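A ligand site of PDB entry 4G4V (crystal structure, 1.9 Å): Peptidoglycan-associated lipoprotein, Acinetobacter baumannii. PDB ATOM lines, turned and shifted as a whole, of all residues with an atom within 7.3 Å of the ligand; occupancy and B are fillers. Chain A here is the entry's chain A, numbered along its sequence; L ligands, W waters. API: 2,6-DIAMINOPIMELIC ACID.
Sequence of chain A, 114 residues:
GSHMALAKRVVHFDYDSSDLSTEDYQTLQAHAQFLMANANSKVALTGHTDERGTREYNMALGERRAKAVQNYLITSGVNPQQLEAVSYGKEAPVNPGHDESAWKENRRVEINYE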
ATOM      1  N   PHE A  13      10.743  -4.433   6.098  1.00  0.00           N
ATOM      2  CA  PHE A  13      11.205  -5.148   7.273  1.00  0.00           C
ATOM      3  C   PHE A  13      10.394  -6.417   7.561  1.00  0.00           C
ATOM      4  O   PHE A  13       9.246  -6.543   7.162  1.00  0.00           O
ATOM      5  CB  PHE A  13      11.114  -4.255   8.513  1.00  0.00           C
ATOM      6  CG  PHE A  13      11.849  -2.955   8.381  1.00  0.00           C
ATOM      7  CD1 PHE A  13      11.253  -1.848   7.759  1.00  0.00           C
ATOM      8  CD2 PHE A  13      13.147  -2.826   8.871  1.00  0.00           C
ATOM      9  CE1 PHE A  13      11.938  -0.646   7.635  1.00  0.00           C
ATOM     10  CE2 PHE A  13      13.846  -1.612   8.747  1.00  0.00           C
ATOM     11  CZ  PHE A  13      13.238  -0.527   8.126  1.00  0.00           C
ATOM     12  N   ASP A  14      11.008  -7.348   8.293  1.00  0.00           N
ATOM     13  CA  ASP A  14      10.342  -8.584   8.672  1.00  0.00           C
ATOM     14  C   ASP A  14       9.522  -8.316   9.943  1.00  0.00           C
ATOM     15  O   ASP A  14       9.663  -7.275  10.586  1.00  0.00           O
ATOM     16  CB  ASP A  14      11.358  -9.684   8.931  1.00  0.00           C
ATOM     17  CG  ASP A  14      12.151 -10.057   7.690  1.00  0.00           C
ATOM     18  OD1 ASP A  14      11.517 -10.296   6.641  1.00  0.00           O
ATOM     19  OD2 ASP A  14      13.394 -10.094   7.765  1.00  0.00           O
ATOM     20  N   TYR A  15       8.657  -9.269  10.276  1.00  0.00           N
ATOM     21  CA  TYR A  15       7.809  -9.157  11.457  1.00  0.00           C
ATOM     22  C   TYR A  15       8.584  -8.803  12.731  1.00  0.00           C
ATOM     23  O   TYR A  15       9.604  -9.406  13.033  1.00  0.00           O
ATOM     24  CB  TYR A  15       7.026 -10.475  11.654  1.00  0.00           C
ATOM     25  CG  TYR A  15       6.183 -10.533  12.901  1.00  0.00           C
ATOM     26  CD1 TYR A  15       6.667 -11.113  14.074  1.00  0.00           C
ATOM     27  CD2 TYR A  15       4.878 -10.029  12.912  1.00  0.00           C
ATOM     28  CE1 TYR A  15       5.880 -11.216  15.216  1.00  0.00           C
ATOM     29  CE2 TYR A  15       4.075 -10.124  14.053  1.00  0.00           C
ATOM     30  CZ  TYR A  15       4.584 -10.721  15.192  1.00  0.00           C
ATOM     31  OH  TYR A  15       3.790 -10.835  16.312  1.00  0.00           O
ATOM     32  N   ASP A  16       8.068  -7.809  13.454  1.00  0.00           N
ATOM     33  CA  ASP A  16       8.647  -7.343  14.705  1.00  0.00           C
ATOM     34  C   ASP A  16      10.145  -7.030  14.627  1.00  0.00           C
ATOM     35  O   ASP A  16      10.842  -7.075  15.644  1.00  0.00           O
ATOM     36  CB  ASP A  16       8.397  -8.366  15.816  1.00  0.00           C
ATOM     37  CG  ASP A  16       8.245  -7.734  17.187  1.00  0.00           C
ATOM     38  OD1 ASP A  16       8.147  -8.494  18.173  1.00  0.00           O
ATOM     39  OD2 ASP A  16       8.225  -6.492  17.276  1.00  0.00           O
ATOM     40  N   SER A  17      10.641  -6.699  13.440  1.00  0.00           N
ATOM     41  CA  SER A  17      12.061  -6.398  13.284  1.00  0.00           C
ATOM     42  C   SER A  17      12.356  -5.038  12.657  1.00  0.00           C
ATOM     43  O   SER A  17      11.607  -4.544  11.818  1.00  0.00           O
ATOM     44  CB  SER A  17      12.713  -7.495  12.442  1.00  0.00           C
ATOM     45  OG  SER A  17      14.086  -7.213  12.237  1.00  0.00           O
ATOM     46  N   HIS A  48       6.639   2.695   9.520  1.00  0.00           N
ATOM     47  CA  HIS A  48       5.316   2.075   9.588  1.00  0.00           C
ATOM     48  C   HIS A  48       5.393   0.605   9.975  1.00  0.00           C
ATOM     49  O   HIS A  48       6.450  -0.017   9.903  1.00  0.00           O
ATOM     50  CB  HIS A  48       4.665   2.183   8.216  1.00  0.00           C
ATOM     51  CG  HIS A  48       4.694   3.555   7.639  1.00  0.00           C
ATOM     52  ND1 HIS A  48       3.660   4.455   7.799  1.00  0.00           N
ATOM     53  CD2 HIS A  48       5.653   4.204   6.935  1.00  0.00           C
ATOM     54  CE1 HIS A  48       3.981   5.597   7.225  1.00  0.00           C
ATOM     55  NE2 HIS A  48       5.177   5.475   6.693  1.00  0.00           N
ATOM     56  N   THR A  49       4.239   0.065  10.374  1.00  0.00           N
ATOM     57  CA  THR A  49       4.128  -1.342  10.754  1.00  0.00           C
ATOM     58  C   THR A  49       2.852  -1.914  10.142  1.00  0.00           C
ATOM     59  O   THR A  49       2.047  -1.182   9.562  1.00  0.00           O
ATOM     60  CB  THR A  49       4.004  -1.523  12.298  1.00  0.00           C
ATOM     61  OG1 THR A  49       2.715  -1.062  12.727  1.00  0.00           O
ATOM     62  CG2 THR A  49       5.076  -0.727  13.020  1.00  0.00           C
ATOM     63  N   ASP A  50       2.676  -3.233  10.231  1.00  0.00           N
ATOM     64  CA  ASP A  50       1.444  -3.807   9.747  1.00  0.00           C
ATOM     65  C   ASP A  50       0.489  -3.691  10.950  1.00  0.00           C
ATOM     66  O   ASP A  50       0.918  -3.370  12.062  1.00  0.00           O
ATOM     67  CB  ASP A  50       1.644  -5.260   9.270  1.00  0.00           C
ATOM     68  CG  ASP A  50       2.125  -6.205  10.364  1.00  0.00           C
ATOM     69  OD1 ASP A  50       2.993  -7.051  10.062  1.00  0.00           O
ATOM     70  OD2 ASP A  50       1.625  -6.123  11.503  1.00  0.00           O
ATOM     71  N   GLU A  51      -0.800  -3.926  10.722  1.00  0.00           N
ATOM     72  CA  GLU A  51      -1.830  -3.793  11.770  1.00  0.00           C
ATOM     73  C   GLU A  51      -1.748  -4.644  13.033  1.00  0.00           C
ATOM     74  O   GLU A  51      -2.476  -4.386  13.986  1.00  0.00           O
ATOM     75  CB  GLU A  51      -3.204  -3.995  11.139  1.00  0.00           C
ATOM     76  CG  GLU A  51      -3.341  -5.309  10.407  1.00  0.00           C
ATOM     77  CD  GLU A  51      -4.704  -5.489   9.777  1.00  0.00           C
ATOM     78  OE1 GLU A  51      -4.818  -6.337   8.862  1.00  0.00           O
ATOM     79  OE2 GLU A  51      -5.649  -4.795  10.194  1.00  0.00           O
ATOM     80  N   ARG A  52      -0.884  -5.647  13.058  1.00  0.00           N
ATOM     81  CA  ARG A  52      -0.778  -6.516  14.229  1.00  0.00           C
ATOM     82  C   ARG A  52      -0.133  -5.868  15.456  1.00  0.00           C
ATOM     83  O   ARG A  52       0.927  -5.257  15.368  1.00  0.00           O
ATOM     84  CB  ARG A  52      -0.017  -7.803  13.848  1.00  0.00           C
ATOM     85  CG  ARG A  52      -0.776  -8.687  12.858  1.00  0.00           C
ATOM     86  CD  ARG A  52       0.028  -9.928  12.427  1.00  0.00           C
ATOM     87  NE  ARG A  52       1.161  -9.589  11.557  1.00  0.00           N
ATOM     88  CZ  ARG A  52       1.936 -10.492  10.959  1.00  0.00           C
ATOM     89  NH1 ARG A  52       1.723 -11.796  11.125  1.00  0.00           N
ATOM     90  NH2 ARG A  52       2.931 -10.092  10.173  1.00  0.00           N
ATOM     91  N   GLY A  53      -0.784  -6.021  16.613  1.00  0.00           N
ATOM     92  CA  GLY A  53      -0.257  -5.441  17.841  1.00  0.00           C
ATOM     93  C   GLY A  53      -0.960  -4.165  18.250  1.00  0.00           C
ATOM     94  O   GLY A  53      -1.792  -3.642  17.503  1.00  0.00           O
ATOM     95  N   THR A  54      -0.625  -3.645  19.423  1.00  0.00           N
ATOM     96  CA  THR A  54      -1.234  -2.415  19.918  1.00  0.00           C
ATOM     97  C   THR A  54      -0.762  -1.192  19.151  1.00  0.00           C
ATOM     98  O   THR A  54       0.270  -1.229  18.470  1.00  0.00           O
ATOM     99  CB  THR A  54      -0.937  -2.210  21.421  1.00  0.00           C
ATOM    100  OG1 THR A  54       0.463  -1.999  21.612  1.00  0.00           O
ATOM    101  CG2 THR A  54      -1.360  -3.425  22.223  1.00  0.00           C
ATOM    102  N   TYR A  57       2.553  -0.213  20.791  1.00  0.00           N
ATOM    103  CA  TYR A  57       3.660  -1.084  20.426  1.00  0.00           C
ATOM    104  C   TYR A  57       4.192  -0.760  19.034  1.00  0.00           C
ATOM    105  O   TYR A  57       5.412  -0.703  18.818  1.00  0.00           O
ATOM    106  CB  TYR A  57       3.228  -2.554  20.439  1.00  0.00           C
ATOM    107  CG  TYR A  57       4.396  -3.494  20.251  1.00  0.00           C
ATOM    108  CD1 TYR A  57       5.103  -3.982  21.345  1.00  0.00           C
ATOM    109  CD2 TYR A  57       4.842  -3.839  18.967  1.00  0.00           C
ATOM    110  CE1 TYR A  57       6.221  -4.778  21.183  1.00  0.00           C
ATOM    111  CE2 TYR A  57       5.968  -4.634  18.799  1.00  0.00           C
ATOM    112  CZ  TYR A  57       6.656  -5.094  19.906  1.00  0.00           C
ATOM    113  OH  TYR A  57       7.785  -5.868  19.758  1.00  0.00           O
ATOM    114  N   ASN A  58       3.285  -0.553  18.100  1.00  0.00           N
ATOM    115  CA  ASN A  58       3.678  -0.260  16.737  1.00  0.00           C
ATOM    116  C   ASN A  58       4.220   1.143  16.526  1.00  0.00           C
ATOM    117  O   ASN A  58       5.020   1.361  15.623  1.00  0.00           O
ATOM    118  CB  ASN A  58       2.536  -0.584  15.783  1.00  0.00           C
ATOM    119  CG  ASN A  58       2.364  -2.078  15.598  1.00  0.00           C
ATOM    120  OD1 ASN A  58       3.324  -2.778  15.265  1.00  0.00           O
ATOM    121  ND2 ASN A  58       1.145  -2.580  15.813  1.00  0.00           N
ATOM    122  N   LEU A  61       7.753   0.627  17.338  1.00  0.00           N
ATOM    123  CA  LEU A  61       8.399  -0.190  16.315  1.00  0.00           C
ATOM    124  C   LEU A  61       8.632   0.657  15.051  1.00  0.00           C
ATOM    125  O   LEU A  61       9.691   0.584  14.420  1.00  0.00           O
ATOM    126  CB  LEU A  61       7.536  -1.415  15.980  1.00  0.00           C
ATOM    127  CG  LEU A  61       7.953  -2.288  14.781  1.00  0.00           C
ATOM    128  CD1 LEU A  61       9.394  -2.739  14.939  1.00  0.00           C
ATOM    129  CD2 LEU A  61       7.016  -3.491  14.672  1.00  0.00           C
ATOM    130  N   GLY A  62       7.639   1.455  14.689  1.00  0.00           N
ATOM    131  CA  GLY A  62       7.787   2.301  13.511  1.00  0.00           C
ATOM    132  C   GLY A  62       8.922   3.282  13.729  1.00  0.00           C
ATOM    133  O   GLY A  62       9.672   3.594  12.803  1.00  0.00           O
ATOM    134  N   ARG A  65      12.246   1.587  13.305  1.00  0.00           N
ATOM    135  CA  ARG A  65      12.509   1.365  11.886  1.00  0.00           C
ATOM    136  C   ARG A  65      13.018   2.635  11.203  1.00  0.00           C
ATOM    137  O   ARG A  65      14.006   2.600  10.465  1.00  0.00           O
ATOM    138  CB  ARG A  65      11.239   0.843  11.188  1.00  0.00           C
ATOM    139  CG  ARG A  65      11.021  -0.662  11.421  1.00  0.00           C
ATOM    140  CD  ARG A  65       9.653  -1.185  10.993  1.00  0.00           C
ATOM    141  NE  ARG A  65       9.599  -2.647  11.098  1.00  0.00           N
ATOM    142  CZ  ARG A  65       8.484  -3.368  11.188  1.00  0.00           C
ATOM    143  NH1 ARG A  65       7.304  -2.785  11.190  1.00  0.00           N
ATOM    144  NH2 ARG A  65       8.560  -4.690  11.297  1.00  0.00           N
ATOM    145  N   GLY A  89       3.199   4.355  13.219  1.00  0.00           N
ATOM    146  CA  GLY A  89       2.731   3.089  13.746  1.00  0.00           C
ATOM    147  C   GLY A  89       2.034   2.264  12.670  1.00  0.00           C
ATOM    148  O   GLY A  89       2.586   2.079  11.582  1.00  0.00           O
ATOM    149  N   LYS A  90       0.827   1.785  12.969  1.00  0.00           N
ATOM    150  CA  LYS A  90       0.055   0.990  12.020  1.00  0.00           C
ATOM    151  C   LYS A  90      -1.087   1.824  11.445  1.00  0.00           C
ATOM    152  O   LYS A  90      -1.984   1.298  10.790  1.00  0.00           O
ATOM    153  CB  LYS A  90      -0.507  -0.257  12.709  1.00  0.00           C
ATOM    154  CG  LYS A  90      -1.439   0.034  13.875  1.00  0.00           C
ATOM    155  CD  LYS A  90      -2.031  -1.260  14.431  1.00  0.00           C
ATOM    156  CE  LYS A  90      -3.052  -0.993  15.519  1.00  0.00           C
ATOM    157  NZ  LYS A  90      -3.796  -2.232  15.876  1.00  0.00           N
ATOM    158  N   TRP A 103       0.605  -7.202   4.766  1.00  0.00           N
ATOM    159  CA  TRP A 103       1.412  -6.784   5.911  1.00  0.00           C
ATOM    160  C   TRP A 103       2.885  -6.651   5.517  1.00  0.00           C
ATOM    161  O   TRP A 103       3.626  -5.895   6.148  1.00  0.00           O
ATOM    162  CB  TRP A 103       1.273  -7.780   7.063  1.00  0.00           C
ATOM    163  CG  TRP A 103      -0.138  -7.943   7.557  1.00  0.00           C
ATOM    164  CD1 TRP A 103      -1.122  -6.998   7.532  1.00  0.00           C
ATOM    165  CD2 TRP A 103      -0.707  -9.102   8.168  1.00  0.00           C
ATOM    166  NE1 TRP A 103      -2.275  -7.496   8.093  1.00  0.00           N
ATOM    167  CE2 TRP A 103      -2.045  -8.791   8.485  1.00  0.00           C
ATOM    168  CE3 TRP A 103      -0.215 -10.379   8.480  1.00  0.00           C
ATOM    169  CZ2 TRP A 103      -2.900  -9.709   9.114  1.00  0.00           C
ATOM    170  CZ3 TRP A 103      -1.071 -11.287   9.096  1.00  0.00           C
ATOM    171  CH2 TRP A 103      -2.392 -10.954   9.406  1.00  0.00           C
ATOM    172  N   ASN A 106       3.208  -3.232   4.233  1.00  0.00           N
ATOM    173  CA  ASN A 106       3.110  -2.212   5.273  1.00  0.00           C
ATOM    174  C   ASN A 106       4.288  -2.075   6.237  1.00  0.00           C
ATOM    175  O   ASN A 106       4.486  -0.987   6.788  1.00  0.00           O
ATOM    176  CB  ASN A 106       1.806  -2.406   6.064  1.00  0.00           C
ATOM    177  CG  ASN A 106       0.564  -2.299   5.181  1.00  0.00           C
ATOM    178  OD1 ASN A 106       0.543  -1.566   4.189  1.00  0.00           O
ATOM    179  ND2 ASN A 106      -0.490  -3.037   5.540  1.00  0.00           N
ATOM    180  N   ARG A 107       5.062  -3.140   6.448  1.00  0.00           N
ATOM    181  CA  ARG A 107       6.228  -3.066   7.321  1.00  0.00           C
ATOM    182  C   ARG A 107       7.291  -2.312   6.509  1.00  0.00           C
ATOM    183  O   ARG A 107       8.043  -2.918   5.759  1.00  0.00           O
ATOM    184  CB  ARG A 107       6.747  -4.481   7.671  1.00  0.00           C
ATOM    185  CG  ARG A 107       5.766  -5.314   8.512  1.00  0.00           C
ATOM    186  CD  ARG A 107       6.435  -6.572   9.057  1.00  0.00           C
ATOM    187  NE  ARG A 107       6.814  -7.520   8.008  1.00  0.00           N
ATOM    188  CZ  ARG A 107       5.957  -8.363   7.420  1.00  0.00           C
ATOM    189  NH1 ARG A 107       4.681  -8.376   7.770  1.00  0.00           N
ATOM    190  NH2 ARG A 107       6.382  -9.182   6.461  1.00  0.00           N
ATOM    191  N   ARG A 108       7.347  -0.997   6.682  1.00  0.00           N
ATOM    192  CA  ARG A 108       8.264  -0.214   5.871  1.00  0.00           C
ATOM    193  C   ARG A 108       8.687   1.140   6.453  1.00  0.00           C
ATOM    194  O   ARG A 108       8.188   1.595   7.487  1.00  0.00           O
ATOM    195  CB  ARG A 108       7.567   0.059   4.532  1.00  0.00           C
ATOM    196  CG  ARG A 108       6.395   1.070   4.698  1.00  0.00           C
ATOM    197  CD  ARG A 108       5.478   1.191   3.490  1.00  0.00           C
ATOM    198  NE  ARG A 108       4.585   2.343   3.582  1.00  0.00           N
ATOM    199  CZ  ARG A 108       3.630   2.496   4.495  1.00  0.00           C
ATOM    200  NH1 ARG A 108       3.409   1.555   5.406  1.00  0.00           N
ATOM    201  NH2 ARG A 108       2.881   3.588   4.496  1.00  0.00           N
HETATM  202  C   API L   1       2.613  -8.437  18.235  1.00  0.00           C
HETATM  203  CA  API L   1       3.850  -7.524  18.319  1.00  0.00           C
HETATM  204  C3  API L   1       4.658  -7.562  16.995  1.00  0.00           C
HETATM  205  C4  API L   1       3.971  -6.922  15.800  1.00  0.00           C
HETATM  206  C5  API L   1       4.918  -6.736  14.600  1.00  0.00           C
HETATM  207  C6  API L   1       4.160  -6.146  13.399  1.00  0.00           C
HETATM  208  C7  API L   1       5.226  -5.555  12.441  1.00  0.00           C
HETATM  209  O   API L   1       2.409  -9.347  19.025  1.00  0.00           O
HETATM  210  OXT API L   1       1.813  -8.134  17.250  1.00  0.00           O
HETATM  211  O3  API L   1       6.334  -6.039  12.296  1.00  0.00           O
HETATM  212  O4  API L   1       4.811  -4.462  11.812  1.00  0.00           O
HETATM  213  N   API L   1       4.603  -8.085  19.449  1.00  0.00           N
HETATM  214  N6  API L   1       3.290  -4.997  13.725  1.00  0.00           N
HETATM  215  O   HOH W   1       5.219 -10.994  18.821  1.00  0.00           O
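The side-chain amide oxygen (OD1) of Asn 58 is in hydrogen-bond range of a nitrogen (N6) of the ligand (2.7 Å). The backbone NH (N) of Asp 16 is in hydrogen-bond range of an oxygen (O3) of the ligand (2.7 Å). OD1 of Asp 16 is in salt-bridge range of N of the ligand (3.8 Å). The guanidinium group (NH2) of Arg 65 is in salt-bridge range of an oxygen (O3) of the ligand (2.8 Å). O of Arg 52 lies within hydrogen-bond range of N6 of the ligand (2.9 Å). The backbone NH (N) of Asp 50 lies within hydrogen-bond range of an oxygen (O4) of the ligand, at 2.9 Å. O of Asp 50 lies within hydrogen-bond range of N6 of the ligand. N6 of the ligand lies within salt-bridge range of OD2 of Asp 50. The side-chain hydroxyl of Tyr 15 sits close to an oxygen (O) of the ligand (3.4 Å). The backbone NH (N) of Gly 53 lies within hydrogen-bond range of an oxygen (OXT) of the ligand (3.4 Å).
OG1 of Thr 49 sits close to OD1 of Asn 58, at 3.1 Å. The backbone carbonyl oxygen of Asp 14 sits at hydrogen-bond distance from the guanidinium group of Arg 65. The guanidinium group (NE) of Arg 65 lies within hydrogen-bond range of the backbone carbonyl oxygen (O) of Ser 17, 2.9 Å away. The backbone NH (N) of Lys 90 lies close to the side-chain hydroxyl (OG1) of Thr 49 (3.4 Å). N of Thr 49 is in hydrogen-bond range of O of Gly 89. NH1 of Arg 107 lies within hydrogen-bond range of O of Trp 103, 3.1 Å away. The backbone carbonyl oxygen (O) of Gly 53 is in hydrogen-bond range of the side-chain amino group (NZ) of Lys 90, at 2.9 Å. The backbone NH of Tyr 57 sits at hydrogen-bond distance from the side-chain hydroxyl of Thr 54 (2.9 Å).
Merely in contact with the ligand: Asp 14, Thr 49, Tyr 57, Leu 61 and Arg 107. 12 residues have an atom within 4 Å of the ligand: Asp 14, Tyr 15, Asp 16, Thr 49, Asp 50, Arg 52, Gly 53, Tyr 57, Asn 58, Leu 61, Arg 65 and Arg 107. The nearest printed residue that does not touch the ligand is Ser 17 (4.5 Å).
Water W1 bridges the side-chain hydroxyl of Tyr 15 (2.9 Å) and a nitrogen (N) of the ligand (3.0 Å).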
